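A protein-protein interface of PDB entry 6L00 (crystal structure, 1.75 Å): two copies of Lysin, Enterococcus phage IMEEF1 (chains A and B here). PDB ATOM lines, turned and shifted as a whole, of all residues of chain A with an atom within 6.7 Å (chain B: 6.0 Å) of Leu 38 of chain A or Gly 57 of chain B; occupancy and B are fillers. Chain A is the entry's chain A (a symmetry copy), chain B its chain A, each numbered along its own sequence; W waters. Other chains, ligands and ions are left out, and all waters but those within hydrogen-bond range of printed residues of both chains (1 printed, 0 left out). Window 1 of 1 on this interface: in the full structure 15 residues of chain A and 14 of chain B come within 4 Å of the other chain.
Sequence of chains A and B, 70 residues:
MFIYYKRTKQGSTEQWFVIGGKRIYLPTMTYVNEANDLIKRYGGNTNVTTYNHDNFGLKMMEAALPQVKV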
ATOM      1  N   MET A   1     -10.684 -16.125 -25.778  1.00  0.00           N
ATOM      2  CA  MET A   1     -11.380 -15.491 -24.662  1.00  0.00           C
ATOM      3  C   MET A   1     -12.393 -16.447 -24.066  1.00  0.00           C
ATOM      4  O   MET A   1     -13.012 -17.226 -24.791  1.00  0.00           O
ATOM      5  CB  MET A   1     -12.097 -14.226 -25.107  1.00  0.00           C
ATOM      6  CG  MET A   1     -12.889 -14.424 -26.373  1.00  0.00           C
ATOM      7  SD  MET A   1     -13.590 -12.908 -27.026  1.00  0.00           S
ATOM      8  CE  MET A   1     -12.431 -11.708 -26.442  1.00  0.00           C
ATOM      9  N   PHE A  17     -12.737 -13.020 -16.594  1.00  0.00           N
ATOM     10  CA  PHE A  17     -12.785 -12.984 -18.051  1.00  0.00           C
ATOM     11  C   PHE A  17     -11.364 -13.011 -18.580  1.00  0.00           C
ATOM     12  O   PHE A  17     -10.568 -12.125 -18.253  1.00  0.00           O
ATOM     13  CB  PHE A  17     -13.513 -11.715 -18.516  1.00  0.00           C
ATOM     14  CG  PHE A  17     -13.573 -11.540 -20.014  1.00  0.00           C
ATOM     15  CD1 PHE A  17     -13.875 -12.601 -20.852  1.00  0.00           C
ATOM     16  CD2 PHE A  17     -13.361 -10.288 -20.577  1.00  0.00           C
ATOM     17  CE1 PHE A  17     -13.965 -12.406 -22.238  1.00  0.00           C
ATOM     18  CE2 PHE A  17     -13.436 -10.094 -21.961  1.00  0.00           C
ATOM     19  CZ  PHE A  17     -13.735 -11.160 -22.788  1.00  0.00           C
ATOM     20  N   ILE A  19      -8.914 -12.571 -21.683  1.00  0.00           N
ATOM     21  CA  ILE A  19      -8.859 -11.927 -22.990  1.00  0.00           C
ATOM     22  C   ILE A  19      -7.453 -11.389 -23.200  1.00  0.00           C
ATOM     23  O   ILE A  19      -6.839 -10.847 -22.278  1.00  0.00           O
ATOM     24  CB  ILE A  19      -9.907 -10.804 -23.102  1.00  0.00           C
ATOM     25  CG1 ILE A  19      -9.735 -10.017 -24.407  1.00  0.00           C
ATOM     26  CG2 ILE A  19      -9.837  -9.890 -21.884  1.00  0.00           C
ATOM     27  CD1 ILE A  19     -10.917  -9.129 -24.723  1.00  0.00           C
ATOM     28  N   THR A  30     -23.485  -6.538 -15.357  1.00  0.00           N
ATOM     29  CA  THR A  30     -23.364  -5.828 -16.628  1.00  0.00           C
ATOM     30  C   THR A  30     -22.006  -6.100 -17.271  1.00  0.00           C
ATOM     31  O   THR A  30     -21.914  -6.266 -18.493  1.00  0.00           O
ATOM     32  CB  THR A  30     -23.591  -4.329 -16.424  1.00  0.00           C
ATOM     33  OG1 THR A  30     -24.906  -4.116 -15.890  1.00  0.00           O
ATOM     34  CG2 THR A  30     -23.476  -3.576 -17.760  1.00  0.00           C
ATOM     35  N   TYR A  31     -20.943  -6.197 -16.463  1.00  0.00           N
ATOM     36  CA  TYR A  31     -19.650  -6.576 -17.032  1.00  0.00           C
ATOM     37  C   TYR A  31     -19.682  -8.010 -17.546  1.00  0.00           C
ATOM     38  O   TYR A  31     -19.128  -8.308 -18.609  1.00  0.00           O
ATOM     39  CB  TYR A  31     -18.534  -6.391 -16.003  1.00  0.00           C
ATOM     40  CG  TYR A  31     -18.012  -4.968 -15.878  1.00  0.00           C
ATOM     41  CD1 TYR A  31     -17.056  -4.476 -16.763  1.00  0.00           C
ATOM     42  CD2 TYR A  31     -18.469  -4.122 -14.872  1.00  0.00           C
ATOM     43  CE1 TYR A  31     -16.575  -3.183 -16.656  1.00  0.00           C
ATOM     44  CE2 TYR A  31     -17.995  -2.827 -14.754  1.00  0.00           C
ATOM     45  CZ  TYR A  31     -17.049  -2.364 -15.648  1.00  0.00           C
ATOM     46  OH  TYR A  31     -16.565  -1.083 -15.530  1.00  0.00           O
ATOM     47  N   ASN A  33     -22.288  -9.643 -18.751  1.00  0.00           N
ATOM     48  CA  ASN A  33     -23.031  -9.627 -20.006  1.00  0.00           C
ATOM     49  C   ASN A  33     -22.174  -9.118 -21.162  1.00  0.00           C
ATOM     50  O   ASN A  33     -22.168  -9.711 -22.247  1.00  0.00           O
ATOM     51  CB  ASN A  33     -24.302  -8.778 -19.848  1.00  0.00           C
ATOM     52  CG  ASN A  33     -25.329  -9.433 -18.926  1.00  0.00           C
ATOM     53  OD1 ASN A  33     -25.252 -10.625 -18.648  1.00  0.00           O
ATOM     54  ND2 ASN A  33     -26.307  -8.650 -18.470  1.00  0.00           N
ATOM     55  N   GLU A  34     -21.425  -8.036 -20.941  1.00  0.00           N
ATOM     56  CA  GLU A  34     -20.621  -7.470 -22.023  1.00  0.00           C
ATOM     57  C   GLU A  34     -19.472  -8.400 -22.401  1.00  0.00           C
ATOM     58  O   GLU A  34     -19.112  -8.499 -23.578  1.00  0.00           O
ATOM     59  CB  GLU A  34     -20.089  -6.091 -21.624  1.00  0.00           C
ATOM     60  CG  GLU A  34     -21.176  -5.017 -21.425  1.00  0.00           C
ATOM     61  CD  GLU A  34     -21.745  -4.502 -22.741  1.00  0.00           C
ATOM     62  OE1 GLU A  34     -21.079  -4.646 -23.796  1.00  0.00           O
ATOM     63  OE2 GLU A  34     -22.866  -3.950 -22.721  1.00  0.00           O
ATOM     64  N   ALA A  35     -18.895  -9.093 -21.416  1.00  0.00           N
ATOM     65  CA  ALA A  35     -17.860 -10.083 -21.701  1.00  0.00           C
ATOM     66  C   ALA A  35     -18.410 -11.228 -22.543  1.00  0.00           C
ATOM     67  O   ALA A  35     -17.784 -11.652 -23.523  1.00  0.00           O
ATOM     68  CB  ALA A  35     -17.265 -10.604 -20.395  1.00  0.00           C
ATOM     69  N   ASN A  36     -19.588 -11.746 -22.182  1.00  0.00           N
ATOM     70  CA  ASN A  36     -20.204 -12.778 -23.009  1.00  0.00           C
ATOM     71  C   ASN A  36     -20.533 -12.257 -24.403  1.00  0.00           C
ATOM     72  O   ASN A  36     -20.411 -12.999 -25.393  1.00  0.00           O
ATOM     73  CB  ASN A  36     -21.456 -13.320 -22.319  1.00  0.00           C
ATOM     74  CG  ASN A  36     -21.149 -14.464 -21.390  1.00  0.00           C
ATOM     75  OD1 ASN A  36     -20.335 -15.337 -21.709  1.00  0.00           O
ATOM     76  ND2 ASN A  36     -21.802 -14.473 -20.231  1.00  0.00           N
ATOM     77  N   ASP A  37     -20.892 -10.975 -24.520  1.00  0.00           N
ATOM     78  CA  ASP A  37     -21.068 -10.401 -25.853  1.00  0.00           C
ATOM     79  C   ASP A  37     -19.769 -10.452 -26.644  1.00  0.00           C
ATOM     80  O   ASP A  37     -19.779 -10.752 -27.845  1.00  0.00           O
ATOM     81  CB  ASP A  37     -21.578  -8.958 -25.759  1.00  0.00           C
ATOM     82  CG  ASP A  37     -23.022  -8.877 -25.286  1.00  0.00           C
ATOM     83  OD1 ASP A  37     -23.731  -9.906 -25.352  1.00  0.00           O
ATOM     84  OD2 ASP A  37     -23.451  -7.787 -24.842  1.00  0.00           O
ATOM     85  N   LEU A  38     -18.637 -10.161 -25.991  1.00  0.00           N
ATOM     86  CA  LEU A  38     -17.351 -10.238 -26.681  1.00  0.00           C
ATOM     87  C   LEU A  38     -17.059 -11.657 -27.134  1.00  0.00           C
ATOM     88  O   LEU A  38     -16.587 -11.882 -28.258  1.00  0.00           O
ATOM     89  CB  LEU A  38     -16.226  -9.738 -25.775  1.00  0.00           C
ATOM     90  CG  LEU A  38     -16.187  -8.236 -25.499  1.00  0.00           C
ATOM     91  CD1 LEU A  38     -15.098  -7.909 -24.477  1.00  0.00           C
ATOM     92  CD2 LEU A  38     -15.976  -7.460 -26.799  1.00  0.00           C
ATOM     93  N   ILE A  39     -17.321 -12.627 -26.260  1.00  0.00           N
ATOM     94  CA  ILE A  39     -17.119 -14.030 -26.594  1.00  0.00           C
ATOM     95  C   ILE A  39     -17.927 -14.413 -27.823  1.00  0.00           C
ATOM     96  O   ILE A  39     -17.433 -15.104 -28.721  1.00  0.00           O
ATOM     97  CB  ILE A  39     -17.488 -14.901 -25.382  1.00  0.00           C
ATOM     98  CG1 ILE A  39     -16.488 -14.648 -24.255  1.00  0.00           C
ATOM     99  CG2 ILE A  39     -17.554 -16.377 -25.776  1.00  0.00           C
ATOM    100  CD1 ILE A  39     -16.737 -15.516 -23.026  1.00  0.00           C
ATOM    101  N   LYS A  40     -19.179 -13.967 -27.882  1.00  0.00           N
ATOM    102  CA  LYS A  40     -20.039 -14.335 -29.002  1.00  0.00           C
ATOM    103  C   LYS A  40     -19.550 -13.712 -30.304  1.00  0.00           C
ATOM    104  O   LYS A  40     -19.615 -14.343 -31.368  1.00  0.00           O
ATOM    105  CB  LYS A  40     -21.481 -13.921 -28.700  1.00  0.00           C
ATOM    106  CG  LYS A  40     -22.426 -13.996 -29.894  1.00  0.00           C
ATOM    107  CD  LYS A  40     -23.376 -15.179 -29.780  1.00  0.00           C
ATOM    108  CE  LYS A  40     -24.217 -15.338 -31.039  1.00  0.00           C
ATOM    109  NZ  LYS A  40     -24.900 -16.657 -31.095  1.00  0.00           N
ATOM    110  N   ARG A  41     -19.027 -12.489 -30.239  1.00  0.00           N
ATOM    111  CA  ARG A  41     -18.629 -11.792 -31.462  1.00  0.00           C
ATOM    112  C   ARG A  41     -17.314 -12.305 -32.032  1.00  0.00           C
ATOM    113  O   ARG A  41     -17.148 -12.345 -33.255  1.00  0.00           O
ATOM    114  CB  ARG A  41     -18.516 -10.299 -31.194  1.00  0.00           C
ATOM    115  CG  ARG A  41     -19.856  -9.675 -30.913  1.00  0.00           C
ATOM    116  CD  ARG A  41     -19.820  -8.184 -31.069  1.00  0.00           C
ATOM    117  NE  ARG A  41     -19.231  -7.545 -29.911  1.00  0.00           N
ATOM    118  CZ  ARG A  41     -19.921  -7.003 -28.913  1.00  0.00           C
ATOM    119  NH1 ARG A  41     -21.250  -7.010 -28.910  1.00  0.00           N
ATOM    120  NH2 ARG A  41     -19.271  -6.462 -27.900  1.00  0.00           N
ATOM    121  N   TYR A  42     -16.363 -12.675 -31.176  1.00  0.00           N
ATOM    122  CA  TYR A  42     -14.988 -12.912 -31.603  1.00  0.00           C
ATOM    123  C   TYR A  42     -14.572 -14.377 -31.472  1.00  0.00           C
ATOM    124  O   TYR A  42     -13.383 -14.679 -31.337  1.00  0.00           O
ATOM    125  CB  TYR A  42     -14.040 -12.005 -30.824  1.00  0.00           C
ATOM    126  CG  TYR A  42     -14.353 -10.530 -31.021  1.00  0.00           C
ATOM    127  CD1 TYR A  42     -14.386  -9.973 -32.297  1.00  0.00           C
ATOM    128  CD2 TYR A  42     -14.637  -9.704 -29.940  1.00  0.00           C
ATOM    129  CE1 TYR A  42     -14.682  -8.625 -32.492  1.00  0.00           C
ATOM    130  CE2 TYR A  42     -14.927  -8.358 -30.122  1.00  0.00           C
ATOM    131  CZ  TYR A  42     -14.937  -7.823 -31.405  1.00  0.00           C
ATOM    132  OH  TYR A  42     -15.236  -6.479 -31.589  1.00  0.00           O
ATOM    133  N   GLY A  43     -15.543 -15.287 -31.512  1.00  0.00           N
ATOM    134  CA  GLY A  43     -15.253 -16.709 -31.551  1.00  0.00           C
ATOM    135  C   GLY A  43     -14.655 -17.266 -30.282  1.00  0.00           C
ATOM    136  O   GLY A  43     -13.862 -18.215 -30.338  1.00  0.00           O
ATOM    137  N   GLY A  44     -15.008 -16.698 -29.136  1.00  0.00           N
ATOM    138  CA  GLY A  44     -14.483 -17.159 -27.877  1.00  0.00           C
ATOM    139  C   GLY A  44     -15.099 -18.478 -27.472  1.00  0.00           C
ATOM    140  O   GLY A  44     -15.995 -19.022 -28.116  1.00  0.00           O
ATOM    141  N   TYR B  51     -18.364   0.417 -30.914  1.00  0.00           N
ATOM    142  CA  TYR B  51     -18.449   0.569 -29.467  1.00  0.00           C
ATOM    143  C   TYR B  51     -18.492   2.040 -29.099  1.00  0.00           C
ATOM    144  O   TYR B  51     -17.581   2.792 -29.460  1.00  0.00           O
ATOM    145  CB  TYR B  51     -17.232  -0.060 -28.794  1.00  0.00           C
ATOM    146  CG  TYR B  51     -17.102  -1.540 -29.008  1.00  0.00           C
ATOM    147  CD1 TYR B  51     -17.628  -2.431 -28.079  1.00  0.00           C
ATOM    148  CD2 TYR B  51     -16.446  -2.052 -30.117  1.00  0.00           C
ATOM    149  CE1 TYR B  51     -17.493  -3.795 -28.254  1.00  0.00           C
ATOM    150  CE2 TYR B  51     -16.310  -3.416 -30.305  1.00  0.00           C
ATOM    151  CZ  TYR B  51     -16.841  -4.283 -29.364  1.00  0.00           C
ATOM    152  OH  TYR B  51     -16.722  -5.642 -29.537  1.00  0.00           O
ATOM    153  N   ASN B  55     -18.606   1.966 -23.376  1.00  0.00           N
ATOM    154  CA  ASN B  55     -19.095   0.595 -23.320  1.00  0.00           C
ATOM    155  C   ASN B  55     -18.130  -0.302 -22.540  1.00  0.00           C
ATOM    156  O   ASN B  55     -16.912  -0.235 -22.713  1.00  0.00           O
ATOM    157  CB  ASN B  55     -19.296   0.056 -24.729  1.00  0.00           C
ATOM    158  CG  ASN B  55     -19.617  -1.419 -24.738  1.00  0.00           C
ATOM    159  OD1 ASN B  55     -18.720  -2.251 -24.826  1.00  0.00           O
ATOM    160  ND2 ASN B  55     -20.899  -1.752 -24.646  1.00  0.00           N
ATOM    161  N   PHE B  56     -18.684  -1.149 -21.669  1.00  0.00           N
ATOM    162  CA  PHE B  56     -17.825  -1.955 -20.800  1.00  0.00           C
ATOM    163  C   PHE B  56     -17.028  -2.989 -21.577  1.00  0.00           C
ATOM    164  O   PHE B  56     -15.909  -3.334 -21.174  1.00  0.00           O
ATOM    165  CB  PHE B  56     -18.654  -2.653 -19.725  1.00  0.00           C
ATOM    166  CG  PHE B  56     -19.217  -1.718 -18.699  1.00  0.00           C
ATOM    167  CD1 PHE B  56     -18.893  -0.371 -18.716  1.00  0.00           C
ATOM    168  CD2 PHE B  56     -20.063  -2.191 -17.704  1.00  0.00           C
ATOM    169  CE1 PHE B  56     -19.408   0.488 -17.772  1.00  0.00           C
ATOM    170  CE2 PHE B  56     -20.580  -1.334 -16.750  1.00  0.00           C
ATOM    171  CZ  PHE B  56     -20.249   0.006 -16.787  1.00  0.00           C
ATOM    172  N   GLY B  57     -17.597  -3.529 -22.656  1.00  0.00           N
ATOM    173  CA  GLY B  57     -16.835  -4.444 -23.498  1.00  0.00           C
ATOM    174  C   GLY B  57     -15.609  -3.780 -24.095  1.00  0.00           C
ATOM    175  O   GLY B  57     -14.497  -4.313 -24.025  1.00  0.00           O
ATOM    176  N   LEU B  58     -15.796  -2.596 -24.689  1.00  0.00           N
ATOM    177  CA  LEU B  58     -14.672  -1.803 -25.182  1.00  0.00           C
ATOM    178  C   LEU B  58     -13.660  -1.531 -24.074  1.00  0.00           C
ATOM    179  O   LEU B  58     -12.441  -1.650 -24.275  1.00  0.00           O
ATOM    180  CB  LEU B  58     -15.181  -0.482 -25.768  1.00  0.00           C
ATOM    181  CG  LEU B  58     -14.071   0.467 -26.215  1.00  0.00           C
ATOM    182  CD1 LEU B  58     -13.244  -0.187 -27.321  1.00  0.00           C
ATOM    183  CD2 LEU B  58     -14.625   1.810 -26.688  1.00  0.00           C
ATOM    184  N   LYS B  59     -14.148  -1.146 -22.897  1.00  0.00           N
ATOM    185  CA  LYS B  59     -13.243  -0.828 -21.800  1.00  0.00           C
ATOM    186  C   LYS B  59     -12.390  -2.029 -21.421  1.00  0.00           C
ATOM    187  O   LYS B  59     -11.201  -1.880 -21.125  1.00  0.00           O
ATOM    188  CB  LYS B  59     -14.034  -0.332 -20.590  1.00  0.00           C
ATOM    189  CG  LYS B  59     -14.683   1.031 -20.799  1.00  0.00           C
ATOM    190  CD  LYS B  59     -13.644   2.127 -20.840  1.00  0.00           C
ATOM    191  CE  LYS B  59     -14.287   3.505 -20.720  1.00  0.00           C
ATOM    192  NZ  LYS B  59     -13.241   4.551 -20.536  1.00  0.00           N
ATOM    193  N   MET B  60     -12.976  -3.227 -21.410  1.00  0.00           N
ATOM    194  CA  MET B  60     -12.175  -4.400 -21.080  1.00  0.00           C
ATOM    195  C   MET B  60     -11.143  -4.683 -22.173  1.00  0.00           C
ATOM    196  O   MET B  60     -10.002  -5.065 -21.882  1.00  0.00           O
ATOM    197  CB  MET B  60     -13.092  -5.599 -20.842  1.00  0.00           C
ATOM    198  CG  MET B  60     -13.924  -5.459 -19.567  1.00  0.00           C
ATOM    199  SD  MET B  60     -14.888  -6.931 -19.137  1.00  0.00           S
ATOM    200  CE  MET B  60     -16.225  -6.800 -20.314  1.00  0.00           C
ATOM    201  N   MET B  61     -11.522  -4.480 -23.437  1.00  0.00           N
ATOM    202  CA  MET B  61     -10.562  -4.649 -24.523  1.00  0.00           C
ATOM    203  C   MET B  61      -9.411  -3.657 -24.397  1.00  0.00           C
ATOM    204  O   MET B  61      -8.241  -4.026 -24.570  1.00  0.00           O
ATOM    205  CB  MET B  61     -11.270  -4.503 -25.870  1.00  0.00           C
ATOM    206  CG  MET B  61     -12.240  -5.646 -26.199  1.00  0.00           C
ATOM    207  SD  MET B  61     -12.408  -5.880 -27.996  1.00  0.00           S
ATOM    208  CE  MET B  61     -13.262  -4.370 -28.399  1.00  0.00           C
ATOM    209  N   GLU B  62      -9.713  -2.397 -24.078  1.00  0.00           N
ATOM    210  CA  GLU B  62      -8.647  -1.406 -23.940  1.00  0.00           C
ATOM    211  C   GLU B  62      -7.761  -1.690 -22.724  1.00  0.00           C
ATOM    212  O   GLU B  62      -6.558  -1.396 -22.754  1.00  0.00           O
ATOM    213  CB  GLU B  62      -9.251  -0.003 -23.868  1.00  0.00           C
ATOM    214  CG  GLU B  62      -9.988   0.417 -25.161  1.00  0.00           C
ATOM    215  CD  GLU B  62     -10.606   1.818 -25.088  1.00  0.00           C
ATOM    216  OE1 GLU B  62     -11.041   2.247 -23.992  1.00  0.00           O
ATOM    217  OE2 GLU B  62     -10.664   2.488 -26.140  1.00  0.00           O
HETATM  218  O   HOH W   1     -21.522  -1.237 -21.119  1.00  0.00           O
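OH of Tyr 51 of chain B sits at hydrogen-bond distance from OH of Tyr 42 of chain A (2.7 Å). The side-chain hydroxyl of Tyr 51 of chain B lies within hydrogen-bond range of the guanidinium group of Arg 41 of chain A, at 3.1 Å. The side-chain carboxylate (OE1) of Glu 34 of chain A lies within hydrogen-bond range of the side-chain amide nitrogen (ND2) of Asn 55 of chain B, 3.0 Å away.
OD1 of Asn 55 of chain B sits at hydrogen-bond distance from N of Leu 58 of chain B (2.9 Å). The backbone NH of Gly 57 of chain B sits at hydrogen-bond distance from the side-chain amide oxygen of Asn 55 of chain B (2.8 Å).
Phe 17 of chain A touches Met 60 of chain B. CG2 of Thr 30 of chain A touches CD2 of Phe 56 of chain B, at 3.7 Å. Tyr 31 of chain A touches Phe 56 of chain B. Tyr 31 of chain A touches Met 60 of chain B. Phe 56 of chain B touches Glu 34 of chain A (CB to CG, 3.9 Å). Glu 34 of chain A touches Gly 57 of chain B. Ala 35 of chain A touches Met 60 of chain B. Tyr 51 of chain B touches Leu 38 of chain A. Leu 38 of chain A touches Gly 57 of chain B (CD1 to O, 3.7 Å).
Of the printed residues of chain B, Leu 38 of chain A touches Tyr 51 (3.4 Å) and Gly 57 (3.7 Å). Of chain A, only Glu 34 (3.7 Å) and Leu 38 (3.7 Å) come within 4 Å of Gly 57 of chain B. Of the printed residues of chain B, Glu 34 of chain A touches Asn 55 (3.0 Å), Phe 56 (3.9 Å) and Gly 57 (3.7 Å). Of the printed residues of chain B, Ala 35 of chain A touches Met 60. Printed residues of chain A within 4 Å of Tyr 51 of chain B: Leu 38 (3.4 Å), Arg 41 (3.1 Å) and Tyr 42 (2.7 Å). The nearest residue of chain B that does not touch Leu 38 of chain A is Met 61 of chain B (4.03 Å). The nearest residue of chain A that does not touch Gly 57 of chain B is Arg 41 of chain A (5.4 Å).
Of the 17 printed residues of chain A, 8 touch a printed residue of chain B. Hydrophobic or aromatic side chains of chain A within 4 Å of the printed part of chain B: Phe 17, Tyr 31, Ala 35, Leu 38 and Tyr 42. Of the 9 printed residues of chain B, 5 touch a printed residue of chain A. Hydrophobic or aromatic side chains of chain B that line the printed part of chain A: Tyr 51, Phe 56 and Met 60. Among the printed residues, 12 pairs touch across the chains.
No position is printed for both chains.
Water W1 lies within hydrogen-bond range of N of Phe 56 of chain B (2.9 Å) and OE2 of Glu 34 of chain A (3.4 Å).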
